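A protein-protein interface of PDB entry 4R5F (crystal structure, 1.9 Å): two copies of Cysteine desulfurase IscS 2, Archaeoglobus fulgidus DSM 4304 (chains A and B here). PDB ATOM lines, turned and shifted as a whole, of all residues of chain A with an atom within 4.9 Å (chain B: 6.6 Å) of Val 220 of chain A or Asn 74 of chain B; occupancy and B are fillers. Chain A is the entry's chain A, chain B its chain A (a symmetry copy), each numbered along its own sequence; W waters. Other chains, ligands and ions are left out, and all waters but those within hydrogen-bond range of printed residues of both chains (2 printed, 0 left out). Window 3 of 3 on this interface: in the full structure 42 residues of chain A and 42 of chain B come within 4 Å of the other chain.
O of Leu 222 of chain A sits at hydrogen-bond distance from ND2 of Asn 74 of chain B, 2.8 Å away.
The backbone carbonyl oxygen of Thr 70 of chain B sits at hydrogen-bond distance from the side-chain amide nitrogen of Asn 74 of chain B (2.9 Å).
The side-chain hydroxyl of Ser 100 of chain B sits at hydrogen-bond distance from the side-chain amide nitrogen of Asn 73 of chain B (2.8 Å).
Among the printed residues, pairs that only touch across the chains: Leu 222 of chain A with Thr 70 of chain B (3.5 Å), Ile 221 of chain A with Thr 70 of chain B (3.6 Å), Asn 74 of chain A with Ile 221 of chain B (3.7 Å), Ile 221 of chain A with Asn 74 of chain B (3.7 Å), Asn 74 of chain A with Val 220 of chain B (3.7 Å), Val 220 of chain A with Asn 74 of chain B (3.7 Å), Leu 222 of chain A with Ser 100 of chain B (3.8 Å), Leu 222 of chain A with Asn 103 of chain B (3.8 Å), Leu 222 of chain A with Pro 104 of chain B (3.8 Å) and Val 220 of chain A with Val 220 of chain B (3.97 Å).
Printed residues of chain B within 4 Å of Asn 74 of chain A: Val 220 (3.7 Å) and Ile 221 (3.7 Å).
Of the printed residues of chain B, Val 220 of chain A touches Asn 74 (3.7 Å) and Val 220 (3.97 Å).
Of the printed residues of chain A, Thr 70 of chain B touches Ile 221 (3.6 Å) and Leu 222 (3.5 Å).
Ala 72 of chain B touches none of the printed residues of chain A.
Printed residues of chain A within 4 Å of Asn 74 of chain B: Val 220, Ile 221 and Leu 222.
Of the printed residues of chain A, Ser 100 of chain B touches Leu 222 (3.8 Å).
Of the printed residues of chain A, Pro 104 of chain B touches Leu 222.
The nearest printed residue of chain B that does not touch Val 220 of chain A is Ile 221 of chain B (4.5 Å).
The nearest printed residue of chain A that does not touch Asn 74 of chain B is Pro 219 of chain A (7.3 Å).
The nearest printed residue of chain A that does not touch Val 220 of chain B is Ile 221 of chain A (4.5 Å).
Of the 10 printed residues of chain A, 4 touch a printed residue of chain B.
Printed residues of chain A that touch a printed residue of chain B: Asn 74, Val 220, Ile 221 and Leu 222.
Hydrophobic or aromatic side chains of chain A that line the printed part of chain B: Val 220, Ile 221 and Leu 222.
Hydrophobic or aromatic side chains of chain B within 4 Å of the printed part of chain A: Pro 104 and Val 220.
Among the printed residues, 11 pairs touch across the chains.
Asn 74 of chain A touches Val 220 of chain B, and with the chains exchanged Val 220 of chain A touches Asn 74 of chain B.
Asn 74 of chain A touches Ile 221 of chain B, and with the chains exchanged Ile 221 of chain A touches Asn 74 of chain B.
Val 220 of chain A touches its own counterpart, Val 220 of chain B.
Water W1 lies within hydrogen-bond range of the side-chain amide oxygen of Asn 74 of chain A and the backbone carbonyl oxygen of Val 220 of chain B.
Water W2 bridges OD1 of Asn 74 of chain B and O of Val 220 of chain A.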
ATOM      1  N   ASN A  74     -13.740  16.289   5.442  1.00  0.00           N
ATOM      2  CA  ASN A  74     -14.763  15.823   4.514  1.00  0.00           C
ATOM      3  C   ASN A  74     -14.725  16.635   3.217  1.00  0.00           C
ATOM      4  O   ASN A  74     -14.845  16.114   2.121  1.00  0.00           O
ATOM      5  CB  ASN A  74     -16.182  15.959   5.125  1.00  0.00           C
ATOM      6  CG  ASN A  74     -16.594  14.780   6.023  1.00  0.00           C
ATOM      7  OD1 ASN A  74     -17.575  14.103   5.731  1.00  0.00           O
ATOM      8  ND2 ASN A  74     -15.849  14.533   7.090  1.00  0.00           N
ATOM      9  N   LEU A  75     -14.623  17.931   3.380  1.00  0.00           N
ATOM     10  CA  LEU A  75     -14.591  18.834   2.232  1.00  0.00           C
ATOM     11  C   LEU A  75     -13.368  18.518   1.366  1.00  0.00           C
ATOM     12  O   LEU A  75     -13.496  18.334   0.137  1.00  0.00           O
ATOM     13  CB  LEU A  75     -14.581  20.285   2.734  1.00  0.00           C
ATOM     14  CG  LEU A  75     -14.392  21.396   1.691  1.00  0.00           C
ATOM     15  CD1 LEU A  75     -15.472  21.314   0.649  1.00  0.00           C
ATOM     16  CD2 LEU A  75     -14.371  22.770   2.356  1.00  0.00           C
ATOM     17  N   ILE A  78     -13.936  14.556  -0.052  1.00  0.00           N
ATOM     18  CA  ILE A  78     -15.066  14.370  -0.928  1.00  0.00           C
ATOM     19  C   ILE A  78     -15.189  15.538  -1.907  1.00  0.00           C
ATOM     20  O   ILE A  78     -15.452  15.306  -3.073  1.00  0.00           O
ATOM     21  CB  ILE A  78     -16.395  14.199  -0.135  1.00  0.00           C
ATOM     22  CG1 ILE A  78     -16.301  12.925   0.705  1.00  0.00           C
ATOM     23  CG2 ILE A  78     -17.570  14.089  -1.100  1.00  0.00           C
ATOM     24  CD1 ILE A  78     -17.386  12.781   1.762  1.00  0.00           C
ATOM     25  N   GLY A  79     -14.991  16.765  -1.433  1.00  0.00           N
ATOM     26  CA  GLY A  79     -15.083  17.938  -2.302  1.00  0.00           C
ATOM     27  C   GLY A  79     -14.091  17.900  -3.447  1.00  0.00           C
ATOM     28  O   GLY A  79     -14.461  18.157  -4.591  1.00  0.00           O
ATOM     29  N   GLN A 218     -15.843  20.775  -4.992  1.00  0.00           N
ATOM     30  CA  GLN A 218     -17.289  20.785  -4.973  1.00  0.00           C
ATOM     31  C   GLN A 218     -17.721  21.003  -3.524  1.00  0.00           C
ATOM     32  O   GLN A 218     -17.192  20.362  -2.598  1.00  0.00           O
ATOM     33  CB  GLN A 218     -17.805  19.456  -5.537  1.00  0.00           C
ATOM     34  CG  GLN A 218     -19.254  19.172  -5.323  1.00  0.00           C
ATOM     35  CD  GLN A 218     -19.660  17.868  -5.986  1.00  0.00           C
ATOM     36  OE1 GLN A 218     -19.314  17.608  -7.146  1.00  0.00           O
ATOM     37  NE2 GLN A 218     -20.375  17.033  -5.248  1.00  0.00           N
ATOM     38  N   PRO A 219     -18.659  21.918  -3.290  1.00  0.00           N
ATOM     39  CA  PRO A 219     -19.048  22.100  -1.889  1.00  0.00           C
ATOM     40  C   PRO A 219     -19.709  20.869  -1.301  1.00  0.00           C
ATOM     41  O   PRO A 219     -20.298  20.087  -2.048  1.00  0.00           O
ATOM     42  CB  PRO A 219     -20.049  23.248  -1.949  1.00  0.00           C
ATOM     43  CG  PRO A 219     -20.529  23.248  -3.332  1.00  0.00           C
ATOM     44  CD  PRO A 219     -19.424  22.784  -4.192  1.00  0.00           C
ATOM     45  N   VAL A 220     -19.606  20.670   0.004  1.00  0.00           N
ATOM     46  CA  VAL A 220     -20.424  19.634   0.632  1.00  0.00           C
ATOM     47  C   VAL A 220     -21.715  20.241   1.206  1.00  0.00           C
ATOM     48  O   VAL A 220     -22.799  19.679   1.031  1.00  0.00           O
ATOM     49  CB  VAL A 220     -19.651  18.894   1.715  1.00  0.00           C
ATOM     50  CG1 VAL A 220     -20.554  17.898   2.428  1.00  0.00           C
ATOM     51  CG2 VAL A 220     -18.467  18.176   1.070  1.00  0.00           C
ATOM     52  N   ILE A 221     -21.605  21.393   1.858  1.00  0.00           N
ATOM     53  CA  ILE A 221     -22.762  21.990   2.522  1.00  0.00           C
ATOM     54  C   ILE A 221     -23.353  23.031   1.561  1.00  0.00           C
ATOM     55  O   ILE A 221     -22.656  23.955   1.152  1.00  0.00           O
ATOM     56  CB  ILE A 221     -22.379  22.618   3.860  1.00  0.00           C
ATOM     57  CG1 ILE A 221     -21.803  21.543   4.806  1.00  0.00           C
ATOM     58  CG2 ILE A 221     -23.572  23.282   4.501  1.00  0.00           C
ATOM     59  CD1 ILE A 221     -22.797  20.404   5.130  1.00  0.00           C
ATOM     60  N   LEU A 222     -24.624  22.848   1.203  1.00  0.00           N
ATOM     61  CA  LEU A 222     -25.269  23.629   0.142  1.00  0.00           C
ATOM     62  C   LEU A 222     -26.253  24.611   0.752  1.00  0.00           C
ATOM     63  O   LEU A 222     -26.883  24.312   1.759  1.00  0.00           O
ATOM     64  CB  LEU A 222     -25.979  22.683  -0.826  1.00  0.00           C
ATOM     65  CG  LEU A 222     -25.103  21.586  -1.436  1.00  0.00           C
ATOM     66  CD1 LEU A 222     -25.889  20.647  -2.295  1.00  0.00           C
ATOM     67  CD2 LEU A 222     -23.977  22.185  -2.236  1.00  0.00           C
ATOM     68  N   LEU A 230     -18.293  27.619  -1.505  1.00  0.00           N
ATOM     69  CA  LEU A 230     -17.766  26.318  -1.105  1.00  0.00           C
ATOM     70  C   LEU A 230     -18.328  25.763   0.187  1.00  0.00           C
ATOM     71  O   LEU A 230     -18.161  24.574   0.455  1.00  0.00           O
ATOM     72  CB  LEU A 230     -16.253  26.371  -0.970  1.00  0.00           C
ATOM     73  CG  LEU A 230     -15.506  26.290  -2.295  1.00  0.00           C
ATOM     74  CD1 LEU A 230     -13.997  26.338  -2.009  1.00  0.00           C
ATOM     75  CD2 LEU A 230     -15.867  25.043  -3.094  1.00  0.00           C
ATOM     76  N   ALA B  69     -28.744  25.785  11.041  1.00  0.00           N
ATOM     77  CA  ALA B  69     -29.902  25.396  10.256  1.00  0.00           C
ATOM     78  C   ALA B  69     -29.513  24.898   8.870  1.00  0.00           C
ATOM     79  O   ALA B  69     -30.164  23.995   8.362  1.00  0.00           O
ATOM     80  CB  ALA B  69     -30.911  26.587  10.142  1.00  0.00           C
ATOM     81  N   THR B  70     -28.474  25.481   8.250  1.00  0.00           N
ATOM     82  CA  THR B  70     -28.118  25.097   6.885  1.00  0.00           C
ATOM     83  C   THR B  70     -27.687  23.645   6.853  1.00  0.00           C
ATOM     84  O   THR B  70     -28.159  22.863   6.038  1.00  0.00           O
ATOM     85  CB  THR B  70     -26.995  26.006   6.289  1.00  0.00           C
ATOM     86  OG1 THR B  70     -27.528  27.312   6.017  1.00  0.00           O
ATOM     87  CG2 THR B  70     -26.464  25.439   5.003  1.00  0.00           C
ATOM     88  N   GLU B  71     -26.759  23.279   7.731  1.00  0.00           N
ATOM     89  CA  GLU B  71     -26.334  21.882   7.827  1.00  0.00           C
ATOM     90  C   GLU B  71     -27.531  20.974   8.155  1.00  0.00           C
ATOM     91  O   GLU B  71     -27.695  19.911   7.561  1.00  0.00           O
ATOM     92  CB  GLU B  71     -25.227  21.714   8.884  1.00  0.00           C
ATOM     93  CG  GLU B  71     -24.635  20.272   8.915  1.00  0.00           C
ATOM     94  CD  GLU B  71     -23.931  19.904  10.229  1.00  0.00           C
ATOM     95  OE1 GLU B  71     -23.436  20.789  10.940  1.00  0.00           O
ATOM     96  OE2 GLU B  71     -23.888  18.704  10.565  1.00  0.00           O
ATOM     97  N   ALA B  72     -28.384  21.389   9.088  1.00  0.00           N
ATOM     98  CA  ALA B  72     -29.542  20.548   9.457  1.00  0.00           C
ATOM     99  C   ALA B  72     -30.484  20.329   8.278  1.00  0.00           C
ATOM    100  O   ALA B  72     -30.938  19.201   8.036  1.00  0.00           O
ATOM    101  CB  ALA B  72     -30.308  21.152  10.610  1.00  0.00           C
ATOM    102  N   ASN B  73     -30.783  21.395   7.535  1.00  0.00           N
ATOM    103  CA  ASN B  73     -31.549  21.252   6.296  1.00  0.00           C
ATOM    104  C   ASN B  73     -30.910  20.331   5.260  1.00  0.00           C
ATOM    105  O   ASN B  73     -31.618  19.558   4.601  1.00  0.00           O
ATOM    106  CB  ASN B  73     -31.801  22.632   5.656  1.00  0.00           C
ATOM    107  CG  ASN B  73     -32.970  23.373   6.283  1.00  0.00           C
ATOM    108  OD1 ASN B  73     -33.884  22.762   6.870  1.00  0.00           O
ATOM    109  ND2 ASN B  73     -32.985  24.699   6.107  1.00  0.00           N
ATOM    110  N   ASN B  74     -29.578  20.417   5.083  1.00  0.00           N
ATOM    111  CA  ASN B  74     -28.875  19.496   4.198  1.00  0.00           C
ATOM    112  C   ASN B  74     -29.059  18.051   4.667  1.00  0.00           C
ATOM    113  O   ASN B  74     -29.271  17.137   3.889  1.00  0.00           O
ATOM    114  CB  ASN B  74     -27.355  19.800   4.161  1.00  0.00           C
ATOM    115  CG  ASN B  74     -26.960  20.905   3.168  1.00  0.00           C
ATOM    116  OD1 ASN B  74     -26.194  20.652   2.243  1.00  0.00           O
ATOM    117  ND2 ASN B  74     -27.484  22.108   3.350  1.00  0.00           N
ATOM    118  N   LEU B  75     -28.905  17.866   5.955  1.00  0.00           N
ATOM    119  CA  LEU B  75     -29.036  16.535   6.545  1.00  0.00           C
ATOM    120  C   LEU B  75     -30.454  16.007   6.308  1.00  0.00           C
ATOM    121  O   LEU B  75     -30.630  14.873   5.814  1.00  0.00           O
ATOM    122  CB  LEU B  75     -28.693  16.612   8.040  1.00  0.00           C
ATOM    123  CG  LEU B  75     -28.917  15.350   8.885  1.00  0.00           C
ATOM    124  CD1 LEU B  75     -28.120  14.206   8.324  1.00  0.00           C
ATOM    125  CD2 LEU B  75     -28.562  15.604  10.348  1.00  0.00           C
ATOM    126  N   ALA B  76     -31.473  16.844   6.582  1.00  0.00           N
ATOM    127  CA  ALA B  76     -32.851  16.409   6.372  1.00  0.00           C
ATOM    128  C   ALA B  76     -33.104  16.012   4.929  1.00  0.00           C
ATOM    129  O   ALA B  76     -33.600  14.933   4.652  1.00  0.00           O
ATOM    130  CB  ALA B  76     -33.840  17.487   6.810  1.00  0.00           C
ATOM    131  N   ILE B  77     -32.718  16.852   3.983  1.00  0.00           N
ATOM    132  CA  ILE B  77     -33.058  16.606   2.593  1.00  0.00           C
ATOM    133  C   ILE B  77     -32.196  15.496   2.009  1.00  0.00           C
ATOM    134  O   ILE B  77     -32.703  14.494   1.454  1.00  0.00           O
ATOM    135  CB  ILE B  77     -32.901  17.923   1.769  1.00  0.00           C
ATOM    136  CG1 ILE B  77     -33.898  18.969   2.262  1.00  0.00           C
ATOM    137  CG2 ILE B  77     -33.044  17.676   0.298  1.00  0.00           C
ATOM    138  CD1 ILE B  77     -35.368  18.577   2.181  1.00  0.00           C
ATOM    139  N   ILE B  78     -30.881  15.662   2.097  1.00  0.00           N
ATOM    140  CA  ILE B  78     -30.017  14.694   1.466  1.00  0.00           C
ATOM    141  C   ILE B  78     -29.917  13.425   2.313  1.00  0.00           C
ATOM    142  O   ILE B  78     -29.958  12.342   1.760  1.00  0.00           O
ATOM    143  CB  ILE B  78     -28.595  15.270   1.202  1.00  0.00           C
ATOM    144  CG1 ILE B  78     -28.715  16.432   0.216  1.00  0.00           C
ATOM    145  CG2 ILE B  78     -27.695  14.190   0.613  1.00  0.00           C
ATOM    146  CD1 ILE B  78     -27.464  17.291   0.093  1.00  0.00           C
ATOM    147  N   GLY B  79     -29.800  13.569   3.631  1.00  0.00           N
ATOM    148  CA  GLY B  79     -29.705  12.408   4.515  1.00  0.00           C
ATOM    149  C   GLY B  79     -30.915  11.500   4.424  1.00  0.00           C
ATOM    150  O   GLY B  79     -30.766  10.285   4.316  1.00  0.00           O
ATOM    151  N   TYR B  80     -32.119  12.067   4.468  1.00  0.00           N
ATOM    152  CA  TYR B  80     -33.292  11.214   4.410  1.00  0.00           C
ATOM    153  C   TYR B  80     -33.464  10.626   3.030  1.00  0.00           C
ATOM    154  O   TYR B  80     -33.786   9.443   2.871  1.00  0.00           O
ATOM    155  CB  TYR B  80     -34.562  11.966   4.818  1.00  0.00           C
ATOM    156  CG  TYR B  80     -35.731  11.028   4.967  1.00  0.00           C
ATOM    157  CD1 TYR B  80     -35.997  10.411   6.183  1.00  0.00           C
ATOM    158  CD2 TYR B  80     -36.551  10.735   3.887  1.00  0.00           C
ATOM    159  CE1 TYR B  80     -37.074   9.539   6.319  1.00  0.00           C
ATOM    160  CE2 TYR B  80     -37.623   9.876   4.009  1.00  0.00           C
ATOM    161  CZ  TYR B  80     -37.876   9.268   5.237  1.00  0.00           C
ATOM    162  OH  TYR B  80     -38.950   8.409   5.376  1.00  0.00           O
ATOM    163  N   MET B  99     -32.815  28.563   0.662  1.00  0.00           N
ATOM    164  CA  MET B  99     -31.881  27.964  -0.296  1.00  0.00           C
ATOM    165  C   MET B  99     -31.134  26.755   0.298  1.00  0.00           C
ATOM    166  O   MET B  99     -30.603  25.919  -0.434  1.00  0.00           O
ATOM    167  CB  MET B  99     -30.847  28.992  -0.769  1.00  0.00           C
ATOM    168  CG  MET B  99     -31.448  30.056  -1.718  1.00  0.00           C
ATOM    169  SD  MET B  99     -32.507  29.298  -2.989  1.00  0.00           S
ATOM    170  CE  MET B  99     -31.249  28.627  -4.026  1.00  0.00           C
ATOM    171  N   SER B 100     -31.068  26.687   1.606  1.00  0.00           N
ATOM    172  CA  SER B 100     -30.425  25.534   2.246  1.00  0.00           C
ATOM    173  C   SER B 100     -31.316  24.281   2.217  1.00  0.00           C
ATOM    174  O   SER B 100     -30.881  23.197   2.622  1.00  0.00           O
ATOM    175  CB  SER B 100     -30.024  25.880   3.670  1.00  0.00           C
ATOM    176  OG  SER B 100     -31.138  26.070   4.532  1.00  0.00           O
ATOM    177  N   VAL B 101     -32.542  24.429   1.726  1.00  0.00           N
ATOM    178  CA  VAL B 101     -33.369  23.291   1.324  1.00  0.00           C
ATOM    179  C   VAL B 101     -33.370  23.128  -0.200  1.00  0.00           C
ATOM    180  O   VAL B 101     -33.241  22.027  -0.716  1.00  0.00           O
ATOM    181  CB  VAL B 101     -34.829  23.460   1.827  1.00  0.00           C
ATOM    182  CG1 VAL B 101     -35.746  22.408   1.248  1.00  0.00           C
ATOM    183  CG2 VAL B 101     -34.848  23.415   3.325  1.00  0.00           C
ATOM    184  N   ASN B 103     -31.168  24.092  -2.602  1.00  0.00           N
ATOM    185  CA  ASN B 103     -29.950  23.653  -3.287  1.00  0.00           C
ATOM    186  C   ASN B 103     -29.622  22.167  -3.012  1.00  0.00           C
ATOM    187  O   ASN B 103     -29.247  21.441  -3.924  1.00  0.00           O
ATOM    188  CB  ASN B 103     -28.806  24.617  -2.931  1.00  0.00           C
ATOM    189  CG  ASN B 103     -28.859  25.871  -3.796  1.00  0.00           C
ATOM    190  OD1 ASN B 103     -29.462  25.838  -4.869  1.00  0.00           O
ATOM    191  ND2 ASN B 103     -28.249  26.964  -3.345  1.00  0.00           N
ATOM    192  N   PRO B 104     -29.860  21.687  -1.787  1.00  0.00           N
ATOM    193  CA  PRO B 104     -29.815  20.226  -1.597  1.00  0.00           C
ATOM    194  C   PRO B 104     -30.829  19.467  -2.462  1.00  0.00           C
ATOM    195  O   PRO B 104     -30.510  18.403  -2.986  1.00  0.00           O
ATOM    196  CB  PRO B 104     -30.120  20.059  -0.109  1.00  0.00           C
ATOM    197  CG  PRO B 104     -29.676  21.304   0.503  1.00  0.00           C
ATOM    198  CD  PRO B 104     -29.804  22.408  -0.512  1.00  0.00           C
ATOM    199  N   THR B 194     -36.101  21.270  11.425  1.00  0.00           N
ATOM    200  CA  THR B 194     -34.914  22.105  11.554  1.00  0.00           C
ATOM    201  C   THR B 194     -35.091  23.222  12.577  1.00  0.00           C
ATOM    202  O   THR B 194     -36.127  23.912  12.608  1.00  0.00           O
ATOM    203  CB  THR B 194     -34.544  22.675  10.210  1.00  0.00           C
ATOM    204  OG1 THR B 194     -34.324  21.582   9.309  1.00  0.00           O
ATOM    205  CG2 THR B 194     -33.298  23.535  10.328  1.00  0.00           C
ATOM    206  N   VAL B 220     -24.395  13.081   6.658  1.00  0.00           N
ATOM    207  CA  VAL B 220     -23.645  13.824   5.647  1.00  0.00           C
ATOM    208  C   VAL B 220     -22.176  13.984   6.075  1.00  0.00           C
ATOM    209  O   VAL B 220     -21.266  13.791   5.266  1.00  0.00           O
ATOM    210  CB  VAL B 220     -24.275  15.182   5.373  1.00  0.00           C
ATOM    211  CG1 VAL B 220     -23.417  15.981   4.401  1.00  0.00           C
ATOM    212  CG2 VAL B 220     -25.674  14.968   4.799  1.00  0.00           C
ATOM    213  N   ILE B 221     -21.947  14.302   7.345  1.00  0.00           N
ATOM    214  CA  ILE B 221     -20.589  14.572   7.814  1.00  0.00           C
ATOM    215  C   ILE B 221     -20.058  13.277   8.443  1.00  0.00           C
ATOM    216  O   ILE B 221     -20.662  12.752   9.372  1.00  0.00           O
ATOM    217  CB  ILE B 221     -20.560  15.730   8.809  1.00  0.00           C
ATOM    218  CG1 ILE B 221     -21.087  17.018   8.142  1.00  0.00           C
ATOM    219  CG2 ILE B 221     -19.161  15.954   9.329  1.00  0.00           C
ATOM    220  CD1 ILE B 221     -20.251  17.473   6.923  1.00  0.00           C
HETATM  221  O   HOH W   1     -19.273  15.391   4.079  1.00  0.00           O
HETATM  222  O   HOH W   2     -24.707  18.448   2.699  1.00  0.00           O
